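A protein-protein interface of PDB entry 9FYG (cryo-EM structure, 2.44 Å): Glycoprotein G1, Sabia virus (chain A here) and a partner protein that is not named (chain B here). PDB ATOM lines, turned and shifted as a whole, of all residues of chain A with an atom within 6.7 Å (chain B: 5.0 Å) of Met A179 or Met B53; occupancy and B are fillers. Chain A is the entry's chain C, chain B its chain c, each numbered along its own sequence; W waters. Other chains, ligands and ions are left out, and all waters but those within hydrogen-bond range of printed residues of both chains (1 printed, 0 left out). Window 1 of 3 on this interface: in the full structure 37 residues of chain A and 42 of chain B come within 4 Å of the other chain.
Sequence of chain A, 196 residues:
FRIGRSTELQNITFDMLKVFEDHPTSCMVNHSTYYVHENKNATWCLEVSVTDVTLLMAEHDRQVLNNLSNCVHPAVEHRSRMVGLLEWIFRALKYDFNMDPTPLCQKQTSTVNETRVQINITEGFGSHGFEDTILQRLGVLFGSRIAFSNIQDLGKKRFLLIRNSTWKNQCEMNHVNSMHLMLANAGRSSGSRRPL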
ATOM      1  N   PHE A  14     -17.488  34.052 -22.304  1.00  0.00           N
ATOM      2  CA  PHE A  14     -16.291  34.133 -23.122  1.00  0.00           C
ATOM      3  C   PHE A  14     -16.573  34.866 -24.431  1.00  0.00           C
ATOM      4  O   PHE A  14     -17.698  34.892 -24.934  1.00  0.00           O
ATOM      5  CB  PHE A  14     -15.746  32.736 -23.415  1.00  0.00           C
ATOM      6  CG  PHE A  14     -14.904  32.170 -22.312  1.00  0.00           C
ATOM      7  CD1 PHE A  14     -13.869  32.907 -21.766  1.00  0.00           C
ATOM      8  CD2 PHE A  14     -15.148  30.902 -21.818  1.00  0.00           C
ATOM      9  CE1 PHE A  14     -13.091  32.386 -20.754  1.00  0.00           C
ATOM     10  CE2 PHE A  14     -14.374  30.379 -20.803  1.00  0.00           C
ATOM     11  CZ  PHE A  14     -13.345  31.122 -20.270  1.00  0.00           C
ATOM     12  N   MET A  16     -15.150  34.565 -28.129  1.00  0.00           N
ATOM     13  CA  MET A  16     -14.387  33.622 -28.932  1.00  0.00           C
ATOM     14  C   MET A  16     -14.050  34.167 -30.315  1.00  0.00           C
ATOM     15  O   MET A  16     -13.691  33.391 -31.207  1.00  0.00           O
ATOM     16  CB  MET A  16     -15.159  32.309 -29.058  1.00  0.00           C
ATOM     17  CG  MET A  16     -15.367  31.577 -27.744  1.00  0.00           C
ATOM     18  SD  MET A  16     -13.820  31.097 -26.964  1.00  0.00           S
ATOM     19  CE  MET A  16     -13.257  29.839 -28.103  1.00  0.00           C
ATOM     20  N   PHE A  20     -11.176  32.667 -33.438  1.00  0.00           N
ATOM     21  CA  PHE A  20     -11.713  32.059 -34.651  1.00  0.00           C
ATOM     22  C   PHE A  20     -11.951  33.065 -35.776  1.00  0.00           C
ATOM     23  O   PHE A  20     -12.699  32.766 -36.711  1.00  0.00           O
ATOM     24  CB  PHE A  20     -13.008  31.308 -34.333  1.00  0.00           C
ATOM     25  CG  PHE A  20     -12.805  30.075 -33.502  1.00  0.00           C
ATOM     26  CD1 PHE A  20     -12.058  29.014 -33.982  1.00  0.00           C
ATOM     27  CD2 PHE A  20     -13.363  29.975 -32.240  1.00  0.00           C
ATOM     28  CE1 PHE A  20     -11.872  27.877 -33.219  1.00  0.00           C
ATOM     29  CE2 PHE A  20     -13.179  28.840 -31.474  1.00  0.00           C
ATOM     30  CZ  PHE A  20     -12.433  27.792 -31.964  1.00  0.00           C
ATOM     31  N   PRO A  24     -11.886  28.877 -40.815  1.00  0.00           N
ATOM     32  CA  PRO A  24     -13.215  28.590 -41.365  1.00  0.00           C
ATOM     33  C   PRO A  24     -14.249  28.420 -40.262  1.00  0.00           C
ATOM     34  O   PRO A  24     -13.980  27.828 -39.216  1.00  0.00           O
ATOM     35  CB  PRO A  24     -13.008  27.287 -42.144  1.00  0.00           C
ATOM     36  CG  PRO A  24     -11.560  27.238 -42.434  1.00  0.00           C
ATOM     37  CD  PRO A  24     -10.866  27.936 -41.312  1.00  0.00           C
ATOM     38  N   ASN A 174     -20.645  30.726 -35.552  1.00  0.00           N
ATOM     39  CA  ASN A 174     -20.785  29.879 -34.377  1.00  0.00           C
ATOM     40  C   ASN A 174     -19.443  29.218 -34.105  1.00  0.00           C
ATOM     41  O   ASN A 174     -18.931  28.481 -34.954  1.00  0.00           O
ATOM     42  CB  ASN A 174     -21.880  28.832 -34.599  1.00  0.00           C
ATOM     43  CG  ASN A 174     -22.430  28.274 -33.308  1.00  0.00           C
ATOM     44  OD1 ASN A 174     -21.779  27.481 -32.635  1.00  0.00           O
ATOM     45  ND2 ASN A 174     -23.643  28.682 -32.958  1.00  0.00           N
ATOM     46  N   HIS A 175     -18.870  29.485 -32.929  1.00  0.00           N
ATOM     47  CA  HIS A 175     -17.552  28.949 -32.616  1.00  0.00           C
ATOM     48  C   HIS A 175     -17.592  27.484 -32.199  1.00  0.00           C
ATOM     49  O   HIS A 175     -16.564  26.808 -32.278  1.00  0.00           O
ATOM     50  CB  HIS A 175     -16.870  29.798 -31.536  1.00  0.00           C
ATOM     51  CG  HIS A 175     -17.304  29.477 -30.140  1.00  0.00           C
ATOM     52  ND1 HIS A 175     -16.616  28.598 -29.331  1.00  0.00           N
ATOM     53  CD2 HIS A 175     -18.342  29.933 -29.402  1.00  0.00           C
ATOM     54  CE1 HIS A 175     -17.222  28.516 -28.160  1.00  0.00           C
ATOM     55  NE2 HIS A 175     -18.272  29.316 -28.177  1.00  0.00           N
ATOM     56  N   VAL A 176     -18.748  26.975 -31.770  1.00  0.00           N
ATOM     57  CA  VAL A 176     -18.908  25.532 -31.611  1.00  0.00           C
ATOM     58  C   VAL A 176     -18.869  24.845 -32.972  1.00  0.00           C
ATOM     59  O   VAL A 176     -18.224  23.801 -33.146  1.00  0.00           O
ATOM     60  CB  VAL A 176     -20.212  25.225 -30.850  1.00  0.00           C
ATOM     61  CG1 VAL A 176     -20.642  23.781 -31.068  1.00  0.00           C
ATOM     62  CG2 VAL A 176     -20.042  25.522 -29.369  1.00  0.00           C
ATOM     63  N   ASN A 177     -19.556  25.426 -33.958  1.00  0.00           N
ATOM     64  CA  ASN A 177     -19.474  24.928 -35.325  1.00  0.00           C
ATOM     65  C   ASN A 177     -18.047  25.012 -35.851  1.00  0.00           C
ATOM     66  O   ASN A 177     -17.572  24.094 -36.532  1.00  0.00           O
ATOM     67  CB  ASN A 177     -20.425  25.718 -36.224  1.00  0.00           C
ATOM     68  CG  ASN A 177     -21.879  25.385 -35.970  1.00  0.00           C
ATOM     69  OD1 ASN A 177     -22.203  24.616 -35.067  1.00  0.00           O
ATOM     70  ND2 ASN A 177     -22.766  25.963 -36.769  1.00  0.00           N
ATOM     71  N   SER A 178     -17.350  26.109 -35.543  1.00  0.00           N
ATOM     72  CA  SER A 178     -15.949  26.240 -35.926  1.00  0.00           C
ATOM     73  C   SER A 178     -15.097  25.156 -35.283  1.00  0.00           C
ATOM     74  O   SER A 178     -14.192  24.611 -35.920  1.00  0.00           O
ATOM     75  CB  SER A 178     -15.422  27.622 -35.539  1.00  0.00           C
ATOM     76  OG  SER A 178     -16.225  28.651 -36.079  1.00  0.00           O
ATOM     77  N   MET A 179     -15.359  24.846 -34.011  1.00  0.00           N
ATOM     78  CA  MET A 179     -14.596  23.806 -33.330  1.00  0.00           C
ATOM     79  C   MET A 179     -14.821  22.444 -33.972  1.00  0.00           C
ATOM     80  O   MET A 179     -13.871  21.676 -34.158  1.00  0.00           O
ATOM     81  CB  MET A 179     -14.959  23.776 -31.846  1.00  0.00           C
ATOM     82  CG  MET A 179     -14.188  24.780 -31.005  1.00  0.00           C
ATOM     83  SD  MET A 179     -14.456  24.604 -29.231  1.00  0.00           S
ATOM     84  CE  MET A 179     -16.193  25.003 -29.105  1.00  0.00           C
ATOM     85  N   HIS A 180     -16.071  22.125 -34.321  1.00  0.00           N
ATOM     86  CA  HIS A 180     -16.338  20.865 -35.014  1.00  0.00           C
ATOM     87  C   HIS A 180     -15.627  20.819 -36.364  1.00  0.00           C
ATOM     88  O   HIS A 180     -14.990  19.812 -36.715  1.00  0.00           O
ATOM     89  CB  HIS A 180     -17.845  20.670 -35.193  1.00  0.00           C
ATOM     90  CG  HIS A 180     -18.541  20.159 -33.970  1.00  0.00           C
ATOM     91  ND1 HIS A 180     -19.288  20.970 -33.143  1.00  0.00           N
ATOM     92  CD2 HIS A 180     -18.606  18.918 -33.435  1.00  0.00           C
ATOM     93  CE1 HIS A 180     -19.778  20.250 -32.151  1.00  0.00           C
ATOM     94  NE2 HIS A 180     -19.380  19.002 -32.305  1.00  0.00           N
ATOM     95  N   LEU A 181     -15.703  21.920 -37.117  1.00  0.00           N
ATOM     96  CA  LEU A 181     -15.075  21.995 -38.432  1.00  0.00           C
ATOM     97  C   LEU A 181     -13.564  21.826 -38.339  1.00  0.00           C
ATOM     98  O   LEU A 181     -12.959  21.117 -39.151  1.00  0.00           O
ATOM     99  CB  LEU A 181     -15.432  23.331 -39.080  1.00  0.00           C
ATOM    100  CG  LEU A 181     -15.172  23.582 -40.561  1.00  0.00           C
ATOM    101  CD1 LEU A 181     -15.783  22.483 -41.406  1.00  0.00           C
ATOM    102  CD2 LEU A 181     -15.729  24.938 -40.947  1.00  0.00           C
ATOM    103  N   MET A 182     -12.937  22.469 -37.354  1.00  0.00           N
ATOM    104  CA  MET A 182     -11.492  22.361 -37.185  1.00  0.00           C
ATOM    105  C   MET A 182     -11.081  20.985 -36.683  1.00  0.00           C
ATOM    106  O   MET A 182     -10.038  20.468 -37.097  1.00  0.00           O
ATOM    107  CB  MET A 182     -10.998  23.439 -36.223  1.00  0.00           C
ATOM    108  CG  MET A 182     -10.880  24.814 -36.846  1.00  0.00           C
ATOM    109  SD  MET A 182     -10.165  26.037 -35.736  1.00  0.00           S
ATOM    110  CE  MET A 182      -8.494  26.123 -36.364  1.00  0.00           C
ATOM    111  N   LEU A 183     -11.866  20.383 -35.785  1.00  0.00           N
ATOM    112  CA  LEU A 183     -11.527  19.058 -35.281  1.00  0.00           C
ATOM    113  C   LEU A 183     -11.568  18.027 -36.396  1.00  0.00           C
ATOM    114  O   LEU A 183     -10.744  17.106 -36.428  1.00  0.00           O
ATOM    115  CB  LEU A 183     -12.469  18.660 -34.145  1.00  0.00           C
ATOM    116  CG  LEU A 183     -12.134  19.238 -32.769  1.00  0.00           C
ATOM    117  CD1 LEU A 183     -13.198  18.882 -31.750  1.00  0.00           C
ATOM    118  CD2 LEU A 183     -10.770  18.761 -32.306  1.00  0.00           C
ATOM    119  N   ALA A 184     -12.518  18.166 -37.322  1.00  0.00           N
ATOM    120  CA  ALA A 184     -12.552  17.263 -38.464  1.00  0.00           C
ATOM    121  C   ALA A 184     -11.437  17.525 -39.469  1.00  0.00           C
ATOM    122  O   ALA A 184     -11.228  16.699 -40.364  1.00  0.00           O
ATOM    123  CB  ALA A 184     -13.903  17.358 -39.165  1.00  0.00           C
ATOM    124  N   GLU B  49     -15.702  21.800 -19.740  1.00  0.00           N
ATOM    125  CA  GLU B  49     -15.584  22.620 -20.940  1.00  0.00           C
ATOM    126  C   GLU B  49     -14.849  23.922 -20.652  1.00  0.00           C
ATOM    127  O   GLU B  49     -14.218  24.493 -21.550  1.00  0.00           O
ATOM    128  CB  GLU B  49     -16.974  22.900 -21.514  1.00  0.00           C
ATOM    129  CG  GLU B  49     -17.766  21.647 -21.864  1.00  0.00           C
ATOM    130  CD  GLU B  49     -18.550  21.088 -20.689  1.00  0.00           C
ATOM    131  OE1 GLU B  49     -19.704  20.666 -20.887  1.00  0.00           O
ATOM    132  OE2 GLU B  49     -18.014  21.072 -19.563  1.00  0.00           O
ATOM    133  N   PHE B  50     -14.919  24.399 -19.407  1.00  0.00           N
ATOM    134  CA  PHE B  50     -14.217  25.619 -19.029  1.00  0.00           C
ATOM    135  C   PHE B  50     -12.708  25.451 -19.139  1.00  0.00           C
ATOM    136  O   PHE B  50     -12.006  26.369 -19.573  1.00  0.00           O
ATOM    137  CB  PHE B  50     -14.609  26.028 -17.609  1.00  0.00           C
ATOM    138  CG  PHE B  50     -13.824  27.189 -17.077  1.00  0.00           C
ATOM    139  CD1 PHE B  50     -14.129  28.481 -17.462  1.00  0.00           C
ATOM    140  CD2 PHE B  50     -12.774  26.986 -16.199  1.00  0.00           C
ATOM    141  CE1 PHE B  50     -13.407  29.548 -16.977  1.00  0.00           C
ATOM    142  CE2 PHE B  50     -12.049  28.050 -15.713  1.00  0.00           C
ATOM    143  CZ  PHE B  50     -12.365  29.334 -16.102  1.00  0.00           C
ATOM    144  N   CYS B  51     -12.187  24.292 -18.737  1.00  0.00           N
ATOM    145  CA  CYS B  51     -10.750  24.061 -18.839  1.00  0.00           C
ATOM    146  C   CYS B  51     -10.308  23.964 -20.294  1.00  0.00           C
ATOM    147  O   CYS B  51      -9.218  24.427 -20.649  1.00  0.00           O
ATOM    148  CB  CYS B  51     -10.369  22.804 -18.059  1.00  0.00           C
ATOM    149  SG  CYS B  51     -10.780  22.895 -16.298  1.00  0.00           S
ATOM    150  N   ASP B  52     -11.145  23.376 -21.152  1.00  0.00           N
ATOM    151  CA  ASP B  52     -10.856  23.371 -22.583  1.00  0.00           C
ATOM    152  C   ASP B  52     -10.823  24.788 -23.141  1.00  0.00           C
ATOM    153  O   ASP B  52      -9.939  25.132 -23.938  1.00  0.00           O
ATOM    154  CB  ASP B  52     -11.894  22.528 -23.322  1.00  0.00           C
ATOM    155  CG  ASP B  52     -11.748  21.048 -23.045  1.00  0.00           C
ATOM    156  OD1 ASP B  52     -10.677  20.636 -22.557  1.00  0.00           O
ATOM    157  OD2 ASP B  52     -12.705  20.295 -23.314  1.00  0.00           O
ATOM    158  N   MET B  53     -11.779  25.627 -22.733  1.00  0.00           N
ATOM    159  CA  MET B  53     -11.778  27.016 -23.178  1.00  0.00           C
ATOM    160  C   MET B  53     -10.541  27.754 -22.682  1.00  0.00           C
ATOM    161  O   MET B  53      -9.961  28.566 -23.410  1.00  0.00           O
ATOM    162  CB  MET B  53     -13.052  27.719 -22.709  1.00  0.00           C
ATOM    163  CG  MET B  53     -14.322  27.244 -23.399  1.00  0.00           C
ATOM    164  SD  MET B  53     -14.419  27.749 -25.126  1.00  0.00           S
ATOM    165  CE  MET B  53     -13.970  26.228 -25.955  1.00  0.00           C
ATOM    166  N   LEU B  54     -10.129  27.491 -21.439  1.00  0.00           N
ATOM    167  CA  LEU B  54      -8.922  28.116 -20.906  1.00  0.00           C
ATOM    168  C   LEU B  54      -7.688  27.690 -21.688  1.00  0.00           C
ATOM    169  O   LEU B  54      -6.813  28.513 -21.975  1.00  0.00           O
ATOM    170  CB  LEU B  54      -8.751  27.771 -19.427  1.00  0.00           C
ATOM    171  CG  LEU B  54      -9.457  28.651 -18.394  1.00  0.00           C
ATOM    172  CD1 LEU B  54      -8.837  28.435 -17.027  1.00  0.00           C
ATOM    173  CD2 LEU B  54      -9.395  30.114 -18.789  1.00  0.00           C
ATOM    174  N   LYS B  55      -7.592  26.403 -22.029  1.00  0.00           N
ATOM    175  CA  LYS B  55      -6.462  25.933 -22.823  1.00  0.00           C
ATOM    176  C   LYS B  55      -6.443  26.594 -24.195  1.00  0.00           C
ATOM    177  O   LYS B  55      -5.383  27.015 -24.678  1.00  0.00           O
ATOM    178  CB  LYS B  55      -6.514  24.413 -22.962  1.00  0.00           C
ATOM    179  CG  LYS B  55      -5.731  23.665 -21.905  1.00  0.00           C
ATOM    180  CD  LYS B  55      -5.611  22.194 -22.258  1.00  0.00           C
ATOM    181  CE  LYS B  55      -6.874  21.435 -21.897  1.00  0.00           C
ATOM    182  NZ  LYS B  55      -7.199  21.567 -20.453  1.00  0.00           N
ATOM    183  N   LEU B  56      -7.610  26.700 -24.834  1.00  0.00           N
ATOM    184  CA  LEU B  56      -7.694  27.364 -26.130  1.00  0.00           C
ATOM    185  C   LEU B  56      -7.262  28.822 -26.033  1.00  0.00           C
ATOM    186  O   LEU B  56      -6.490  29.313 -26.867  1.00  0.00           O
ATOM    187  CB  LEU B  56      -9.120  27.260 -26.672  1.00  0.00           C
ATOM    188  CG  LEU B  56      -9.330  27.396 -28.180  1.00  0.00           C
ATOM    189  CD1 LEU B  56      -8.411  26.460 -28.939  1.00  0.00           C
ATOM    190  CD2 LEU B  56     -10.782  27.129 -28.536  1.00  0.00           C
ATOM    191  N   PHE B  57      -7.750  29.530 -25.012  1.00  0.00           N
ATOM    192  CA  PHE B  57      -7.410  30.940 -24.858  1.00  0.00           C
ATOM    193  C   PHE B  57      -5.929  31.125 -24.565  1.00  0.00           C
ATOM    194  O   PHE B  57      -5.305  32.060 -25.073  1.00  0.00           O
ATOM    195  CB  PHE B  57      -8.260  31.574 -23.759  1.00  0.00           C
ATOM    196  CG  PHE B  57      -9.506  32.228 -24.268  1.00  0.00           C
ATOM    197  CD1 PHE B  57     -10.751  31.753 -23.905  1.00  0.00           C
ATOM    198  CD2 PHE B  57      -9.433  33.313 -25.121  1.00  0.00           C
ATOM    199  CE1 PHE B  57     -11.897  32.352 -24.382  1.00  0.00           C
ATOM    200  CE2 PHE B  57     -10.577  33.914 -25.599  1.00  0.00           C
ATOM    201  CZ  PHE B  57     -11.810  33.434 -25.227  1.00  0.00           C
ATOM    202  N   GLU B  58      -5.347  30.250 -23.744  1.00  0.00           N
ATOM    203  CA  GLU B  58      -3.920  30.347 -23.453  1.00  0.00           C
ATOM    204  C   GLU B  58      -3.082  30.096 -24.701  1.00  0.00           C
ATOM    205  O   GLU B  58      -2.105  30.814 -24.952  1.00  0.00           O
ATOM    206  CB  GLU B  58      -3.547  29.371 -22.338  1.00  0.00           C
ATOM    207  CG  GLU B  58      -2.063  29.327 -22.004  1.00  0.00           C
ATOM    208  CD  GLU B  58      -1.496  30.685 -21.631  1.00  0.00           C
ATOM    209  OE1 GLU B  58      -2.236  31.512 -21.061  1.00  0.00           O
ATOM    210  OE2 GLU B  58      -0.303  30.926 -21.909  1.00  0.00           O
ATOM    211  N   ILE B  86      -8.997  20.997 -27.237  1.00  0.00           N
ATOM    212  CA  ILE B  86     -10.433  20.755 -27.178  1.00  0.00           C
ATOM    213  C   ILE B  86     -10.664  19.253 -27.209  1.00  0.00           C
ATOM    214  O   ILE B  86     -10.195  18.566 -28.124  1.00  0.00           O
ATOM    215  CB  ILE B  86     -11.167  21.448 -28.340  1.00  0.00           C
ATOM    216  CG1 ILE B  86     -11.136  22.966 -28.160  1.00  0.00           C
ATOM    217  CG2 ILE B  86     -12.596  20.944 -28.451  1.00  0.00           C
ATOM    218  CD1 ILE B  86     -11.692  23.435 -26.843  1.00  0.00           C
ATOM    219  N   LEU B  91     -17.066  17.581 -26.699  1.00  0.00           N
ATOM    220  CA  LEU B  91     -17.797  18.352 -27.698  1.00  0.00           C
ATOM    221  C   LEU B  91     -18.870  17.504 -28.369  1.00  0.00           C
ATOM    222  O   LEU B  91     -19.988  17.976 -28.607  1.00  0.00           O
ATOM    223  CB  LEU B  91     -16.821  18.915 -28.732  1.00  0.00           C
ATOM    224  CG  LEU B  91     -17.294  20.076 -29.605  1.00  0.00           C
ATOM    225  CD1 LEU B  91     -17.311  21.377 -28.820  1.00  0.00           C
ATOM    226  CD2 LEU B  91     -16.424  20.206 -30.838  1.00  0.00           C
ATOM    227  N   TYR B 107     -20.472  26.245 -24.639  1.00  0.00           N
ATOM    228  CA  TYR B 107     -19.094  26.731 -24.530  1.00  0.00           C
ATOM    229  C   TYR B 107     -19.006  28.254 -24.501  1.00  0.00           C
ATOM    230  O   TYR B 107     -18.013  28.835 -24.942  1.00  0.00           O
ATOM    231  CB  TYR B 107     -18.221  26.168 -25.657  1.00  0.00           C
ATOM    232  CG  TYR B 107     -17.956  24.684 -25.540  1.00  0.00           C
ATOM    233  CD1 TYR B 107     -18.946  23.756 -25.830  1.00  0.00           C
ATOM    234  CD2 TYR B 107     -16.716  24.212 -25.133  1.00  0.00           C
ATOM    235  CE1 TYR B 107     -18.709  22.405 -25.719  1.00  0.00           C
ATOM    236  CE2 TYR B 107     -16.469  22.861 -25.022  1.00  0.00           C
ATOM    237  CZ  TYR B 107     -17.470  21.961 -25.317  1.00  0.00           C
ATOM    238  OH  TYR B 107     -17.227  20.614 -25.204  1.00  0.00           O
ATOM    239  N   PHE B 110     -20.167  30.350 -18.283  1.00  0.00           N
ATOM    240  CA  PHE B 110     -19.778  29.426 -17.228  1.00  0.00           C
ATOM    241  C   PHE B 110     -20.059  30.049 -15.870  1.00  0.00           C
ATOM    242  O   PHE B 110     -19.751  31.220 -15.641  1.00  0.00           O
ATOM    243  CB  PHE B 110     -18.296  29.047 -17.342  1.00  0.00           C
ATOM    244  CG  PHE B 110     -17.951  28.345 -18.623  1.00  0.00           C
ATOM    245  CD1 PHE B 110     -17.688  29.064 -19.777  1.00  0.00           C
ATOM    246  CD2 PHE B 110     -17.905  26.965 -18.678  1.00  0.00           C
ATOM    247  CE1 PHE B 110     -17.384  28.417 -20.955  1.00  0.00           C
ATOM    248  CE2 PHE B 110     -17.603  26.316 -19.856  1.00  0.00           C
ATOM    249  CZ  PHE B 110     -17.339  27.044 -20.993  1.00  0.00           C
HETATM  250  O   HOH W   1     -10.462  30.333 -26.633  1.00  0.00           O
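Of the 15 printed residues of chain A, 7 touch a printed residue of chain B.
Hydrophobic or aromatic side chains of chain A within 4 Å of the printed part of chain B: Phe A14, Met A16, Phe A20, His A175, Met A179, His A180 and Leu A183.
Along chain A the printed residues that touch a printed residue of chain B span positions 14 to 183.
Of the 14 printed residues of chain B, 8 touch a printed residue of chain A.
Hydrophobic or aromatic side chains of chain B within 4 Å of the printed part of chain A: Phe B50, Met B53, Leu B56, Phe B57, Ile B86, Leu B91, Tyr B107 and Phe B110.
O of Tyr B107 lies within hydrogen-bond range of NE2 of His A175.
The side-chain hydroxyl (OH) of Tyr B107 sits at hydrogen-bond distance from the backbone NH (N) of Leu B91, 3.4 Å away.
A ring nitrogen (ND1) of His A180 lies within hydrogen-bond range of the backbone carbonyl oxygen (O) of Val A176 (3.0 Å).
Water W1 bridges the backbone NH of Phe B57 (3.3 Å) and the side-chain sulfur of Met A16 (3.5 Å).
Of the printed residues of chain B, His A175 touches Tyr B107 (3.3 Å).
Asn A177 touches none of the printed residues of chain B.
Of the printed residues of chain B, Met A179 touches Met B53 (3.7 Å), Ile B86 (3.8 Å), Leu B91 (3.8 Å) and Tyr B107 (3.99 Å).
Printed residues of chain B within 4 Å of His A180: Leu B91 (3.5 Å).
Met B53 touches just these residues of chain A: Phe A14 (3.5 Å), Met A16 (3.8 Å) and Met A179 (3.7 Å).
Of the printed residues of chain A, Phe B57 touches Phe A14 (3.3 Å) and Met A16 (3.5 Å).
Glu B58 touches none of the printed residues of chain A.
The nearest printed residue of chain A that does not touch Ile B86 is Phe A20 (6.3 Å).
Met B53 touches Phe A14.
Phe B57 touches Phe A14 (CE1 to CD1, 3.3 Å).
CE of Met A16 touches SD of Met B53, at 3.8 Å.
CE of Met A16 touches CD2 of Leu B56 (3.7 Å).
Phe B57 touches Met A16.
CD2 of Leu B56 touches CZ of Phe A20, 3.9 Å away.
CE of Met B53 touches SD of Met A179, 3.7 Å away.
Met A179 touches Leu B91.
Tyr B107 touches Met A179 (CG to CE, 3.99 Å).
Leu B91 touches Leu A183 (CD2 to CD1, 3.6 Å).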
